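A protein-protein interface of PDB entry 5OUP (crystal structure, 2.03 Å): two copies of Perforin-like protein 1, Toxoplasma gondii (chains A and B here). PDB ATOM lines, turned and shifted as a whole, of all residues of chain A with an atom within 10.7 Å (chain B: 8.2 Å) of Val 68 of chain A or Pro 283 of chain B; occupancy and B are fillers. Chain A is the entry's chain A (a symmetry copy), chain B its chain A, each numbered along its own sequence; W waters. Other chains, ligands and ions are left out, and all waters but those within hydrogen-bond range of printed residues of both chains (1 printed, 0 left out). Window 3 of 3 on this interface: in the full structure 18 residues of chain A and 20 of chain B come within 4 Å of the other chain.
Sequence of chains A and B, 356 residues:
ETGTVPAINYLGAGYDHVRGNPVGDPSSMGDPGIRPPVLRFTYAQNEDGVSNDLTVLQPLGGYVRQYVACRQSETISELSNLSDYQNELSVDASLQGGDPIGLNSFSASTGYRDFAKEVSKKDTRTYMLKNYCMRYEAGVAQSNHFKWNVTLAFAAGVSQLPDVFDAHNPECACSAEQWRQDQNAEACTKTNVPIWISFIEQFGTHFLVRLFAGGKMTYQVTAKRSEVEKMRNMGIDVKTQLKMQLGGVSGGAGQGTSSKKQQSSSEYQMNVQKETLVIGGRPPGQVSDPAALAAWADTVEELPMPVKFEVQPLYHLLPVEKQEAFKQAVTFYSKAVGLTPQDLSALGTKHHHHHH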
ATOM      1  N   ARG A  65      -4.585  25.945 -12.247  1.00  0.00           N
ATOM      2  CA  ARG A  65      -5.591  24.987 -12.690  1.00  0.00           C
ATOM      3  C   ARG A  65      -6.945  25.426 -12.145  1.00  0.00           C
ATOM      4  O   ARG A  65      -7.192  25.348 -10.938  1.00  0.00           O
ATOM      5  CB  ARG A  65      -5.236  23.577 -12.231  1.00  0.00           C
ATOM      6  CG  ARG A  65      -6.193  22.511 -12.719  1.00  0.00           C
ATOM      7  CD  ARG A  65      -5.554  21.140 -12.645  1.00  0.00           C
ATOM      8  NE  ARG A  65      -6.504  20.082 -12.966  1.00  0.00           N
ATOM      9  CZ  ARG A  65      -7.198  19.408 -12.056  1.00  0.00           C
ATOM     10  NH1 ARG A  65      -7.044  19.680 -10.767  1.00  0.00           N
ATOM     11  NH2 ARG A  65      -8.043  18.460 -12.433  1.00  0.00           N
ATOM     12  N   GLN A  66      -7.816  25.886 -13.037  1.00  0.00           N
ATOM     13  CA  GLN A  66      -9.123  26.401 -12.660  1.00  0.00           C
ATOM     14  C   GLN A  66     -10.136  25.264 -12.590  1.00  0.00           C
ATOM     15  O   GLN A  66     -10.110  24.343 -13.412  1.00  0.00           O
ATOM     16  CB  GLN A  66      -9.573  27.460 -13.666  1.00  0.00           C
ATOM     17  CG  GLN A  66     -10.761  28.292 -13.236  1.00  0.00           C
ATOM     18  CD  GLN A  66     -11.044  29.418 -14.210  1.00  0.00           C
ATOM     19  OE1 GLN A  66     -10.307  29.614 -15.178  1.00  0.00           O
ATOM     20  NE2 GLN A  66     -12.113  30.165 -13.960  1.00  0.00           N
ATOM     21  N   TYR A  67     -11.020  25.330 -11.602  1.00  0.00           N
ATOM     22  CA  TYR A  67     -12.026  24.301 -11.375  1.00  0.00           C
ATOM     23  C   TYR A  67     -13.362  24.705 -11.987  1.00  0.00           C
ATOM     24  O   TYR A  67     -13.619  25.879 -12.263  1.00  0.00           O
ATOM     25  CB  TYR A  67     -12.206  24.041  -9.877  1.00  0.00           C
ATOM     26  CG  TYR A  67     -10.997  23.448  -9.192  1.00  0.00           C
ATOM     27  CD1 TYR A  67     -10.080  22.681  -9.898  1.00  0.00           C
ATOM     28  CD2 TYR A  67     -10.777  23.653  -7.836  1.00  0.00           C
ATOM     29  CE1 TYR A  67      -8.977  22.132  -9.273  1.00  0.00           C
ATOM     30  CE2 TYR A  67      -9.676  23.111  -7.203  1.00  0.00           C
ATOM     31  CZ  TYR A  67      -8.782  22.351  -7.924  1.00  0.00           C
ATOM     32  OH  TYR A  67      -7.689  21.808  -7.292  1.00  0.00           O
ATOM     33  N   VAL A  68     -14.213  23.706 -12.199  1.00  0.00           N
ATOM     34  CA  VAL A  68     -15.599  23.928 -12.591  1.00  0.00           C
ATOM     35  C   VAL A  68     -16.407  24.113 -11.316  1.00  0.00           C
ATOM     36  O   VAL A  68     -16.431  23.226 -10.451  1.00  0.00           O
ATOM     37  CB  VAL A  68     -16.138  22.756 -13.426  1.00  0.00           C
ATOM     38  CG1 VAL A  68     -17.630  22.903 -13.647  1.00  0.00           C
ATOM     39  CG2 VAL A  68     -15.405  22.660 -14.760  1.00  0.00           C
ATOM     40  N   ALA A  69     -17.065  25.269 -11.198  1.00  0.00           N
ATOM     41  CA  ALA A  69     -17.762  25.656  -9.976  1.00  0.00           C
ATOM     42  C   ALA A  69     -16.801  25.570  -8.795  1.00  0.00           C
ATOM     43  O   ALA A  69     -15.763  26.244  -8.785  1.00  0.00           O
ATOM     44  CB  ALA A  69     -19.002  24.788  -9.756  1.00  0.00           C
ATOM     45  N   CYS A  70     -17.128  24.739  -7.810  1.00  0.00           N
ATOM     46  CA  CYS A  70     -16.328  24.602  -6.605  1.00  0.00           C
ATOM     47  C   CYS A  70     -16.083  23.130  -6.331  1.00  0.00           C
ATOM     48  O   CYS A  70     -16.991  22.301  -6.440  1.00  0.00           O
ATOM     49  CB  CYS A  70     -17.005  25.267  -5.396  1.00  0.00           C
ATOM     50  SG  CYS A  70     -18.683  24.705  -5.036  1.00  0.00           S
ATOM     51  N   ARG A  71     -14.828  22.822  -6.021  1.00  0.00           N
ATOM     52  CA  ARG A  71     -14.405  21.501  -5.581  1.00  0.00           C
ATOM     53  C   ARG A  71     -14.686  21.400  -4.088  1.00  0.00           C
ATOM     54  O   ARG A  71     -14.057  22.095  -3.284  1.00  0.00           O
ATOM     55  CB  ARG A  71     -12.922  21.309  -5.888  1.00  0.00           C
ATOM     56  CG  ARG A  71     -12.371  19.956  -5.522  1.00  0.00           C
ATOM     57  CD  ARG A  71     -10.865  19.882  -5.767  1.00  0.00           C
ATOM     58  NE  ARG A  71     -10.353  18.521  -5.624  1.00  0.00           N
ATOM     59  CZ  ARG A  71      -9.067  18.190  -5.716  1.00  0.00           C
ATOM     60  NH1 ARG A  71      -8.156  19.125  -5.948  1.00  0.00           N
ATOM     61  NH2 ARG A  71      -8.694  16.924  -5.574  1.00  0.00           N
ATOM     62  N   GLN A  72     -15.631  20.545  -3.714  1.00  0.00           N
ATOM     63  CA  GLN A  72     -16.179  20.531  -2.366  1.00  0.00           C
ATOM     64  C   GLN A  72     -15.582  19.390  -1.555  1.00  0.00           C
ATOM     65  O   GLN A  72     -15.507  18.251  -2.030  1.00  0.00           O
ATOM     66  CB  GLN A  72     -17.701  20.410  -2.408  1.00  0.00           C
ATOM     67  CG  GLN A  72     -18.354  21.434  -3.323  1.00  0.00           C
ATOM     68  CD  GLN A  72     -19.781  21.743  -2.929  1.00  0.00           C
ATOM     69  OE1 GLN A  72     -20.682  20.933  -3.134  1.00  0.00           O
ATOM     70  NE2 GLN A  72     -19.993  22.924  -2.358  1.00  0.00           N
ATOM     71  N   TYR A 132     -14.820  23.120   2.667  1.00  0.00           N
ATOM     72  CA  TYR A 132     -13.975  23.730   1.647  1.00  0.00           C
ATOM     73  C   TYR A 132     -14.763  24.003   0.373  1.00  0.00           C
ATOM     74  O   TYR A 132     -15.509  23.145  -0.109  1.00  0.00           O
ATOM     75  CB  TYR A 132     -12.790  22.831   1.293  1.00  0.00           C
ATOM     76  CG  TYR A 132     -11.799  22.544   2.396  1.00  0.00           C
ATOM     77  CD1 TYR A 132     -12.054  21.565   3.350  1.00  0.00           C
ATOM     78  CD2 TYR A 132     -10.581  23.211   2.449  1.00  0.00           C
ATOM     79  CE1 TYR A 132     -11.135  21.279   4.342  1.00  0.00           C
ATOM     80  CE2 TYR A 132      -9.655  22.930   3.437  1.00  0.00           C
ATOM     81  CZ  TYR A 132      -9.937  21.964   4.379  1.00  0.00           C
ATOM     82  OH  TYR A 132      -9.016  21.682   5.360  1.00  0.00           O
ATOM     83  N   CYS A 133     -14.561  25.196  -0.191  1.00  0.00           N
ATOM     84  CA  CYS A 133     -15.154  25.606  -1.468  1.00  0.00           C
ATOM     85  C   CYS A 133     -14.010  26.073  -2.375  1.00  0.00           C
ATOM     86  O   CYS A 133     -13.789  27.272  -2.551  1.00  0.00           O
ATOM     87  CB  CYS A 133     -16.205  26.698  -1.250  1.00  0.00           C
ATOM     88  SG  CYS A 133     -16.955  27.347  -2.754  1.00  0.00           S
ATOM     89  N   MET A 134     -13.286  25.116  -2.953  1.00  0.00           N
ATOM     90  CA  MET A 134     -12.078  25.410  -3.717  1.00  0.00           C
ATOM     91  C   MET A 134     -12.419  25.753  -5.162  1.00  0.00           C
ATOM     92  O   MET A 134     -13.192  25.043  -5.814  1.00  0.00           O
ATOM     93  CB  MET A 134     -11.117  24.223  -3.673  1.00  0.00           C
ATOM     94  CG  MET A 134     -10.496  23.982  -2.308  1.00  0.00           C
ATOM     95  SD  MET A 134      -9.516  22.471  -2.276  1.00  0.00           S
ATOM     96  CE  MET A 134     -10.812  21.236  -2.353  1.00  0.00           C
ATOM     97  N   ARG A 135     -11.816  26.830  -5.666  1.00  0.00           N
ATOM     98  CA  ARG A 135     -12.067  27.304  -7.020  1.00  0.00           C
ATOM     99  C   ARG A 135     -10.903  27.102  -7.976  1.00  0.00           C
ATOM    100  O   ARG A 135     -11.135  26.957  -9.179  1.00  0.00           O
ATOM    101  CB  ARG A 135     -12.436  28.792  -6.999  1.00  0.00           C
ATOM    102  CG  ARG A 135     -13.820  29.065  -6.448  1.00  0.00           C
ATOM    103  CD  ARG A 135     -14.663  29.777  -7.484  1.00  0.00           C
ATOM    104  NE  ARG A 135     -14.899  28.952  -8.662  1.00  0.00           N
ATOM    105  CZ  ARG A 135     -15.187  29.436  -9.867  1.00  0.00           C
ATOM    106  NH1 ARG A 135     -15.389  28.611 -10.884  1.00  0.00           N
ATOM    107  NH2 ARG A 135     -15.259  30.747 -10.056  1.00  0.00           N
ATOM    108  N   TYR A 136      -9.663  27.099  -7.491  1.00  0.00           N
ATOM    109  CA  TYR A 136      -8.534  26.802  -8.364  1.00  0.00           C
ATOM    110  C   TYR A 136      -7.350  26.353  -7.518  1.00  0.00           C
ATOM    111  O   TYR A 136      -7.331  26.510  -6.296  1.00  0.00           O
ATOM    112  CB  TYR A 136      -8.160  28.002  -9.247  1.00  0.00           C
ATOM    113  CG  TYR A 136      -7.581  29.196  -8.515  1.00  0.00           C
ATOM    114  CD1 TYR A 136      -6.227  29.256  -8.204  1.00  0.00           C
ATOM    115  CD2 TYR A 136      -8.381  30.275  -8.163  1.00  0.00           C
ATOM    116  CE1 TYR A 136      -5.691  30.347  -7.543  1.00  0.00           C
ATOM    117  CE2 TYR A 136      -7.851  31.374  -7.507  1.00  0.00           C
ATOM    118  CZ  TYR A 136      -6.506  31.401  -7.202  1.00  0.00           C
ATOM    119  OH  TYR A 136      -5.972  32.485  -6.545  1.00  0.00           O
ATOM    120  N   GLU A 137      -6.361  25.783  -8.202  1.00  0.00           N
ATOM    121  CA  GLU A 137      -5.097  25.380  -7.606  1.00  0.00           C
ATOM    122  C   GLU A 137      -3.960  26.055  -8.360  1.00  0.00           C
ATOM    123  O   GLU A 137      -4.022  26.208  -9.584  1.00  0.00           O
ATOM    124  CB  GLU A 137      -4.925  23.857  -7.646  1.00  0.00           C
ATOM    125  CG  GLU A 137      -3.603  23.362  -7.083  1.00  0.00           C
ATOM    126  CD  GLU A 137      -3.253  21.962  -7.547  1.00  0.00           C
ATOM    127  OE1 GLU A 137      -3.939  21.447  -8.454  1.00  0.00           O
ATOM    128  OE2 GLU A 137      -2.289  21.380  -7.008  1.00  0.00           O
ATOM    129  N   ALA A 213      -7.239  27.754  -3.663  1.00  0.00           N
ATOM    130  CA  ALA A 213      -7.901  29.010  -3.356  1.00  0.00           C
ATOM    131  C   ALA A 213      -9.405  28.879  -3.534  1.00  0.00           C
ATOM    132  O   ALA A 213      -9.888  28.134  -4.392  1.00  0.00           O
ATOM    133  CB  ALA A 213      -7.375  30.145  -4.239  1.00  0.00           C
ATOM    134  N   GLU A 301     -16.587  32.993  -5.649  1.00  0.00           N
ATOM    135  CA  GLU A 301     -16.142  33.050  -7.039  1.00  0.00           C
ATOM    136  C   GLU A 301     -15.457  34.375  -7.346  1.00  0.00           C
ATOM    137  O   GLU A 301     -14.502  34.416  -8.130  1.00  0.00           O
ATOM    138  CB  GLU A 301     -17.326  32.837  -7.987  1.00  0.00           C
ATOM    139  CG  GLU A 301     -17.786  31.389  -8.128  1.00  0.00           C
ATOM    140  CD  GLU A 301     -18.699  30.941  -7.006  1.00  0.00           C
ATOM    141  OE1 GLU A 301     -19.896  31.300  -7.035  1.00  0.00           O
ATOM    142  OE2 GLU A 301     -18.220  30.230  -6.097  1.00  0.00           O
ATOM    143  N   ASP B  25     -13.140  14.662 -12.246  1.00  0.00           N
ATOM    144  CA  ASP B  25     -12.021  15.585 -12.206  1.00  0.00           C
ATOM    145  C   ASP B  25     -12.572  16.937 -11.786  1.00  0.00           C
ATOM    146  O   ASP B  25     -13.679  17.289 -12.213  1.00  0.00           O
ATOM    147  CB  ASP B  25     -11.343  15.680 -13.578  1.00  0.00           C
ATOM    148  CG  ASP B  25     -10.032  16.436 -13.533  1.00  0.00           C
ATOM    149  OD1 ASP B  25      -8.978  15.785 -13.378  1.00  0.00           O
ATOM    150  OD2 ASP B  25     -10.056  17.681 -13.648  1.00  0.00           O
ATOM    151  N   PRO B  26     -11.862  17.707 -10.958  1.00  0.00           N
ATOM    152  CA  PRO B  26     -12.416  19.001 -10.525  1.00  0.00           C
ATOM    153  C   PRO B  26     -12.489  20.036 -11.636  1.00  0.00           C
ATOM    154  O   PRO B  26     -13.191  21.042 -11.473  1.00  0.00           O
ATOM    155  CB  PRO B  26     -11.459  19.442  -9.409  1.00  0.00           C
ATOM    156  CG  PRO B  26     -10.183  18.729  -9.700  1.00  0.00           C
ATOM    157  CD  PRO B  26     -10.575  17.409 -10.307  1.00  0.00           C
ATOM    158  N   SER B  27     -11.800  19.829 -12.756  1.00  0.00           N
ATOM    159  CA  SER B  27     -11.796  20.793 -13.847  1.00  0.00           C
ATOM    160  C   SER B  27     -12.730  20.403 -14.985  1.00  0.00           C
ATOM    161  O   SER B  27     -12.754  21.086 -16.014  1.00  0.00           O
ATOM    162  CB  SER B  27     -10.373  20.980 -14.373  1.00  0.00           C
ATOM    163  OG  SER B  27      -9.572  21.635 -13.405  1.00  0.00           O
ATOM    164  N   SER B  28     -13.506  19.336 -14.821  1.00  0.00           N
ATOM    165  CA  SER B  28     -14.422  18.870 -15.851  1.00  0.00           C
ATOM    166  C   SER B  28     -15.718  18.405 -15.204  1.00  0.00           C
ATOM    167  O   SER B  28     -15.736  17.985 -14.044  1.00  0.00           O
ATOM    168  CB  SER B  28     -13.812  17.727 -16.674  1.00  0.00           C
ATOM    169  OG  SER B  28     -14.724  17.256 -17.650  1.00  0.00           O
ATOM    170  N   MET B  29     -16.809  18.492 -15.961  1.00  0.00           N
ATOM    171  CA  MET B  29     -18.056  17.894 -15.508  1.00  0.00           C
ATOM    172  C   MET B  29     -18.159  16.423 -15.878  1.00  0.00           C
ATOM    173  O   MET B  29     -19.096  15.751 -15.429  1.00  0.00           O
ATOM    174  CB  MET B  29     -19.254  18.660 -16.074  1.00  0.00           C
ATOM    175  CG  MET B  29     -19.573  19.944 -15.325  1.00  0.00           C
ATOM    176  SD  MET B  29     -19.755  19.678 -13.549  1.00  0.00           S
ATOM    177  CE  MET B  29     -21.087  18.484 -13.509  1.00  0.00           C
ATOM    178  N   GLY B  30     -17.224  15.910 -16.673  1.00  0.00           N
ATOM    179  CA  GLY B  30     -17.220  14.507 -17.029  1.00  0.00           C
ATOM    180  C   GLY B  30     -15.868  13.862 -16.806  1.00  0.00           C
ATOM    181  O   GLY B  30     -14.999  14.439 -16.143  1.00  0.00           O
ATOM    182  N   MET B 217     -22.327  10.651  -8.551  1.00  0.00           N
ATOM    183  CA  MET B 217     -21.765  11.379  -7.423  1.00  0.00           C
ATOM    184  C   MET B 217     -20.991  10.385  -6.570  1.00  0.00           C
ATOM    185  O   MET B 217     -21.569   9.413  -6.070  1.00  0.00           O
ATOM    186  CB  MET B 217     -22.862  12.068  -6.613  1.00  0.00           C
ATOM    187  CG  MET B 217     -22.329  12.978  -5.522  1.00  0.00           C
ATOM    188  SD  MET B 217     -23.363  14.432  -5.292  1.00  0.00           S
ATOM    189  CE  MET B 217     -23.246  15.185  -6.914  1.00  0.00           C
ATOM    190  N   VAL B 278     -18.087  14.588  -8.942  1.00  0.00           N
ATOM    191  CA  VAL B 278     -19.366  14.566  -9.645  1.00  0.00           C
ATOM    192  C   VAL B 278     -19.121  14.399 -11.141  1.00  0.00           C
ATOM    193  O   VAL B 278     -18.242  15.054 -11.714  1.00  0.00           O
ATOM    194  CB  VAL B 278     -20.188  15.837  -9.355  1.00  0.00           C
ATOM    195  CG1 VAL B 278     -19.352  17.087  -9.577  1.00  0.00           C
ATOM    196  CG2 VAL B 278     -21.454  15.869 -10.200  1.00  0.00           C
ATOM    197  N   GLY B 280     -21.543  14.502 -14.669  1.00  0.00           N
ATOM    198  CA  GLY B 280     -22.836  14.692 -15.289  1.00  0.00           C
ATOM    199  C   GLY B 280     -23.638  15.818 -14.662  1.00  0.00           C
ATOM    200  O   GLY B 280     -23.388  16.261 -13.541  1.00  0.00           O
ATOM    201  N   GLY B 281     -24.633  16.276 -15.417  1.00  0.00           N
ATOM    202  CA  GLY B 281     -25.497  17.348 -14.979  1.00  0.00           C
ATOM    203  C   GLY B 281     -24.776  18.685 -14.948  1.00  0.00           C
ATOM    204  O   GLY B 281     -23.684  18.865 -15.490  1.00  0.00           O
ATOM    205  N   ARG B 282     -25.429  19.639 -14.297  1.00  0.00           N
ATOM    206  CA  ARG B 282     -24.844  20.951 -14.093  1.00  0.00           C
ATOM    207  C   ARG B 282     -23.998  20.960 -12.828  1.00  0.00           C
ATOM    208  O   ARG B 282     -24.140  20.088 -11.965  1.00  0.00           O
ATOM    209  CB  ARG B 282     -25.942  22.011 -14.016  1.00  0.00           C
ATOM    210  CG  ARG B 282     -26.314  22.574 -15.374  1.00  0.00           C
ATOM    211  CD  ARG B 282     -27.035  23.908 -15.269  1.00  0.00           C
ATOM    212  NE  ARG B 282     -26.879  24.683 -16.497  1.00  0.00           N
ATOM    213  CZ  ARG B 282     -27.560  24.453 -17.614  1.00  0.00           C
ATOM    214  NH1 ARG B 282     -28.445  23.470 -17.656  1.00  0.00           N
ATOM    215  NH2 ARG B 282     -27.355  25.202 -18.689  1.00  0.00           N
ATOM    216  N   PRO B 283     -23.078  21.915 -12.707  1.00  0.00           N
ATOM    217  CA  PRO B 283     -22.240  21.998 -11.505  1.00  0.00           C
ATOM    218  C   PRO B 283     -23.085  22.147 -10.253  1.00  0.00           C
ATOM    219  O   PRO B 283     -23.968  23.017 -10.188  1.00  0.00           O
ATOM    220  CB  PRO B 283     -21.392  23.252 -11.757  1.00  0.00           C
ATOM    221  CG  PRO B 283     -21.340  23.379 -13.232  1.00  0.00           C
ATOM    222  CD  PRO B 283     -22.663  22.888 -13.735  1.00  0.00           C
ATOM    223  N   PRO B 284     -22.848  21.313  -9.240  1.00  0.00           N
ATOM    224  CA  PRO B 284     -23.654  21.381  -8.012  1.00  0.00           C
ATOM    225  C   PRO B 284     -23.087  22.357  -6.992  1.00  0.00           C
ATOM    226  O   PRO B 284     -21.889  22.337  -6.699  1.00  0.00           O
ATOM    227  CB  PRO B 284     -23.615  19.936  -7.500  1.00  0.00           C
ATOM    228  CG  PRO B 284     -22.279  19.436  -7.945  1.00  0.00           C
ATOM    229  CD  PRO B 284     -21.940  20.150  -9.241  1.00  0.00           C
ATOM    230  N   GLY B 285     -23.947  23.214  -6.442  1.00  0.00           N
ATOM    231  CA  GLY B 285     -23.469  24.243  -5.535  1.00  0.00           C
ATOM    232  C   GLY B 285     -23.041  23.700  -4.185  1.00  0.00           C
ATOM    233  O   GLY B 285     -21.989  24.076  -3.659  1.00  0.00           O
ATOM    234  N   GLN B 286     -23.844  22.812  -3.602  1.00  0.00           N
ATOM    235  CA  GLN B 286     -23.575  22.298  -2.264  1.00  0.00           C
ATOM    236  C   GLN B 286     -23.994  20.840  -2.191  1.00  0.00           C
ATOM    237  O   GLN B 286     -25.176  20.523  -2.351  1.00  0.00           O
ATOM    238  CB  GLN B 286     -24.308  23.120  -1.201  1.00  0.00           C
ATOM    239  CG  GLN B 286     -23.828  22.855   0.209  1.00  0.00           C
ATOM    240  CD  GLN B 286     -22.334  23.068   0.355  1.00  0.00           C
ATOM    241  OE1 GLN B 286     -21.759  23.971  -0.255  1.00  0.00           O
ATOM    242  NE2 GLN B 286     -21.695  22.228   1.162  1.00  0.00           N
ATOM    243  N   ALA B 292     -29.817  21.365  -2.808  1.00  0.00           N
ATOM    244  CA  ALA B 292     -28.867  21.535  -3.904  1.00  0.00           C
ATOM    245  C   ALA B 292     -28.521  20.203  -4.562  1.00  0.00           C
ATOM    246  O   ALA B 292     -28.272  20.159  -5.772  1.00  0.00           O
ATOM    247  CB  ALA B 292     -27.602  22.232  -3.403  1.00  0.00           C
ATOM    248  N   ALA B 295     -31.521  19.348  -6.849  1.00  0.00           N
ATOM    249  CA  ALA B 295     -31.492  20.168  -8.055  1.00  0.00           C
ATOM    250  C   ALA B 295     -30.460  19.656  -9.049  1.00  0.00           C
ATOM    251  O   ALA B 295     -30.670  19.748 -10.264  1.00  0.00           O
ATOM    252  CB  ALA B 295     -31.210  21.626  -7.693  1.00  0.00           C
ATOM    253  N   TRP B 296     -29.346  19.107  -8.554  1.00  0.00           N
ATOM    254  CA  TRP B 296     -28.337  18.557  -9.454  1.00  0.00           C
ATOM    255  C   TRP B 296     -28.889  17.383 -10.249  1.00  0.00           C
ATOM    256  O   TRP B 296     -28.645  17.274 -11.458  1.00  0.00           O
ATOM    257  CB  TRP B 296     -27.096  18.129  -8.672  1.00  0.00           C
ATOM    258  CG  TRP B 296     -26.162  17.285  -9.491  1.00  0.00           C
ATOM    259  CD1 TRP B 296     -25.295  17.717 -10.453  1.00  0.00           C
ATOM    260  CD2 TRP B 296     -26.010  15.861  -9.429  1.00  0.00           C
ATOM    261  NE1 TRP B 296     -24.614  16.654 -10.993  1.00  0.00           N
ATOM    262  CE2 TRP B 296     -25.035  15.502 -10.381  1.00  0.00           C
ATOM    263  CE3 TRP B 296     -26.606  14.855  -8.662  1.00  0.00           C
ATOM    264  CZ2 TRP B 296     -24.638  14.180 -10.583  1.00  0.00           C
ATOM    265  CZ3 TRP B 296     -26.211  13.545  -8.862  1.00  0.00           C
ATOM    266  CH2 TRP B 296     -25.237  13.218  -9.816  1.00  0.00           C
ATOM    267  N   THR B 299     -30.818  18.418 -13.119  1.00  0.00           N
ATOM    268  CA  THR B 299     -29.973  18.836 -14.230  1.00  0.00           C
ATOM    269  C   THR B 299     -29.301  17.659 -14.924  1.00  0.00           C
ATOM    270  O   THR B 299     -28.830  17.813 -16.056  1.00  0.00           O
ATOM    271  CB  THR B 299     -28.908  19.824 -13.748  1.00  0.00           C
ATOM    272  OG1 THR B 299     -28.051  19.180 -12.797  1.00  0.00           O
ATOM    273  CG2 THR B 299     -29.563  21.037 -13.099  1.00  0.00           C
ATOM    274  N   LEU B 303     -28.337  17.248 -18.913  1.00  0.00           N
ATOM    275  CA  LEU B 303     -26.959  17.081 -19.377  1.00  0.00           C
ATOM    276  C   LEU B 303     -26.403  15.741 -18.910  1.00  0.00           C
ATOM    277  O   LEU B 303     -25.528  15.685 -18.038  1.00  0.00           O
ATOM    278  CB  LEU B 303     -26.080  18.231 -18.884  1.00  0.00           C
ATOM    279  CG  LEU B 303     -26.474  19.624 -19.372  1.00  0.00           C
ATOM    280  CD1 LEU B 303     -25.655  20.689 -18.665  1.00  0.00           C
ATOM    281  CD2 LEU B 303     -26.300  19.718 -20.878  1.00  0.00           C
ATOM    282  N   MET B 305     -24.104  12.417 -19.040  1.00  0.00           N
ATOM    283  CA  MET B 305     -22.761  12.149 -19.526  1.00  0.00           C
ATOM    284  C   MET B 305     -22.353  10.742 -19.146  1.00  0.00           C
ATOM    285  O   MET B 305     -22.930  10.145 -18.223  1.00  0.00           O
ATOM    286  CB  MET B 305     -21.767  13.183 -18.982  1.00  0.00           C
ATOM    287  CG  MET B 305     -21.812  14.474 -19.777  1.00  0.00           C
ATOM    288  SD  MET B 305     -20.491  15.619 -19.382  1.00  0.00           S
ATOM    289  CE  MET B 305     -21.108  16.271 -17.848  1.00  0.00           C
HETATM  290  O   HOH W   1     -14.910  21.215  -9.097  1.00  0.00           O
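The side-chain carboxylate (OD2) of Asp 25 of chain B lies within hydrogen-bond range of the backbone NH (N) of Ser 27 of chain B (2.9 Å). O of Met 29 of chain B lies within hydrogen-bond range of N of Gly 280 of chain B (2.9 Å). The guanidinium group (NE) of Arg 135 of chain A lies within hydrogen-bond range of the backbone carbonyl oxygen (O) of Ala 69 of chain A (2.8 Å). The backbone carbonyl oxygen (O) of Glu 137 of chain A is in hydrogen-bond range of the backbone NH (N) of Arg 65 of chain A. NE2 of Gln 72 of chain A is in hydrogen-bond range of SG of Cys 70 of chain A, 3.5 Å away. The side-chain hydroxyl (OG) of Ser 28 of chain B sits at hydrogen-bond distance from the backbone NH (N) of Gly 30 of chain B.
Of chain B, only Pro 26, Ser 27, Ser 28, Met 29 and Pro 283 come within 4 Å of Val 68 of chain A. Ala 69 of chain A touches just one residue of chain B: Pro 283. Of the printed residues of chain B, Gln 72 of chain A touches Gly 285 (2.6 Å) and Gln 286 (2.9 Å). Printed residues of chain A within 4 Å of Asp 25 of chain B: Arg 65. Ser 28 of chain B touches just one residue of chain A: Val 68. Printed residues of chain A within 4 Å of Met 29 of chain B: Val 68. Of chain A, only Val 68 and Ala 69 come within 4 Å of Pro 283 of chain B. The nearest residue of chain B that does not touch Val 68 of chain A is Asp 25 of chain B (6.1 Å). The nearest residue of chain A that does not touch Pro 283 of chain B is Cys 70 of chain A (6.0 Å).
O of Pro 26 of chain B lies within hydrogen-bond range of N of Val 68 of chain A (2.9 Å). O of Gly 285 of chain B lies within hydrogen-bond range of NE2 of Gln 72 of chain A, 2.6 Å away. The guanidinium group (NH2) of Arg 65 of chain A is in salt-bridge range of the side-chain carboxylate (OD2) of Asp 25 of chain B (2.5 Å). The side-chain hydroxyl (OG) of Ser 27 of chain B lies within hydrogen-bond range of the backbone carbonyl oxygen (O) of Gln 66 of chain A (2.8 Å). OE1 of Gln 286 of chain B lies within hydrogen-bond range of NE2 of Gln 72 of chain A (2.9 Å). The side-chain hydroxyl of Ser 27 of chain B is in hydrogen-bond range of the guanidinium group of Arg 65 of chain A. O of Gly 285 of chain B is in hydrogen-bond range of SG of Cys 70 of chain A (3.6 Å).
Pro 26 of chain B touches Arg 65 of chain A (CG to NH1, 3.4 Å). Pro 26 of chain B touches Tyr 67 of chain A. Tyr 67 of chain A touches Ser 27 of chain B. CG2 of Val 68 of chain A touches O of Ser 27 of chain B, at 3.3 Å. CG2 of Val 68 of chain A touches N of Ser 28 of chain B, 3.8 Å away. Val 68 of chain A touches Met 29 of chain B. Pro 283 of chain B touches Val 68 of chain A (CG to CG1, 3.8 Å). Pro 283 of chain B touches Ala 69 of chain A. Arg 71 of chain A touches Pro 26 of chain B.
Water W1 lies within hydrogen-bond range of the backbone carbonyl oxygen of Val 68 of chain A (2.9 Å), the backbone carbonyl oxygen of Pro 26 of chain B (2.9 Å) and the backbone NH of Arg 71 of chain A (3.5 Å).
Of the 16 printed residues of chain A, 8 touch a printed residue of chain B. Hydrophobic or aromatic side chains of chain A within 4 Å of the printed part of chain B: Tyr 67, Val 68 and Ala 69. Of the 21 printed residues of chain B, 8 touch a printed residue of chain A. Printed residues of chain B that touch a printed residue of chain A: Asp 25, Pro 26, Ser 27, Ser 28, Met 29, Pro 283, Gly 285 and Gln 286. Among the printed residues, Asp or Glu carboxylates within 4 Å of a Lys or Arg side-chain nitrogen of the other chain: Arg 65 of chain A with Asp 25 of chain B (2.5 Å).
No position is printed for both chains. Of the 16 pairs that touch across the chains among the printed residues, none has its exchanged pair printed and touching as well.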
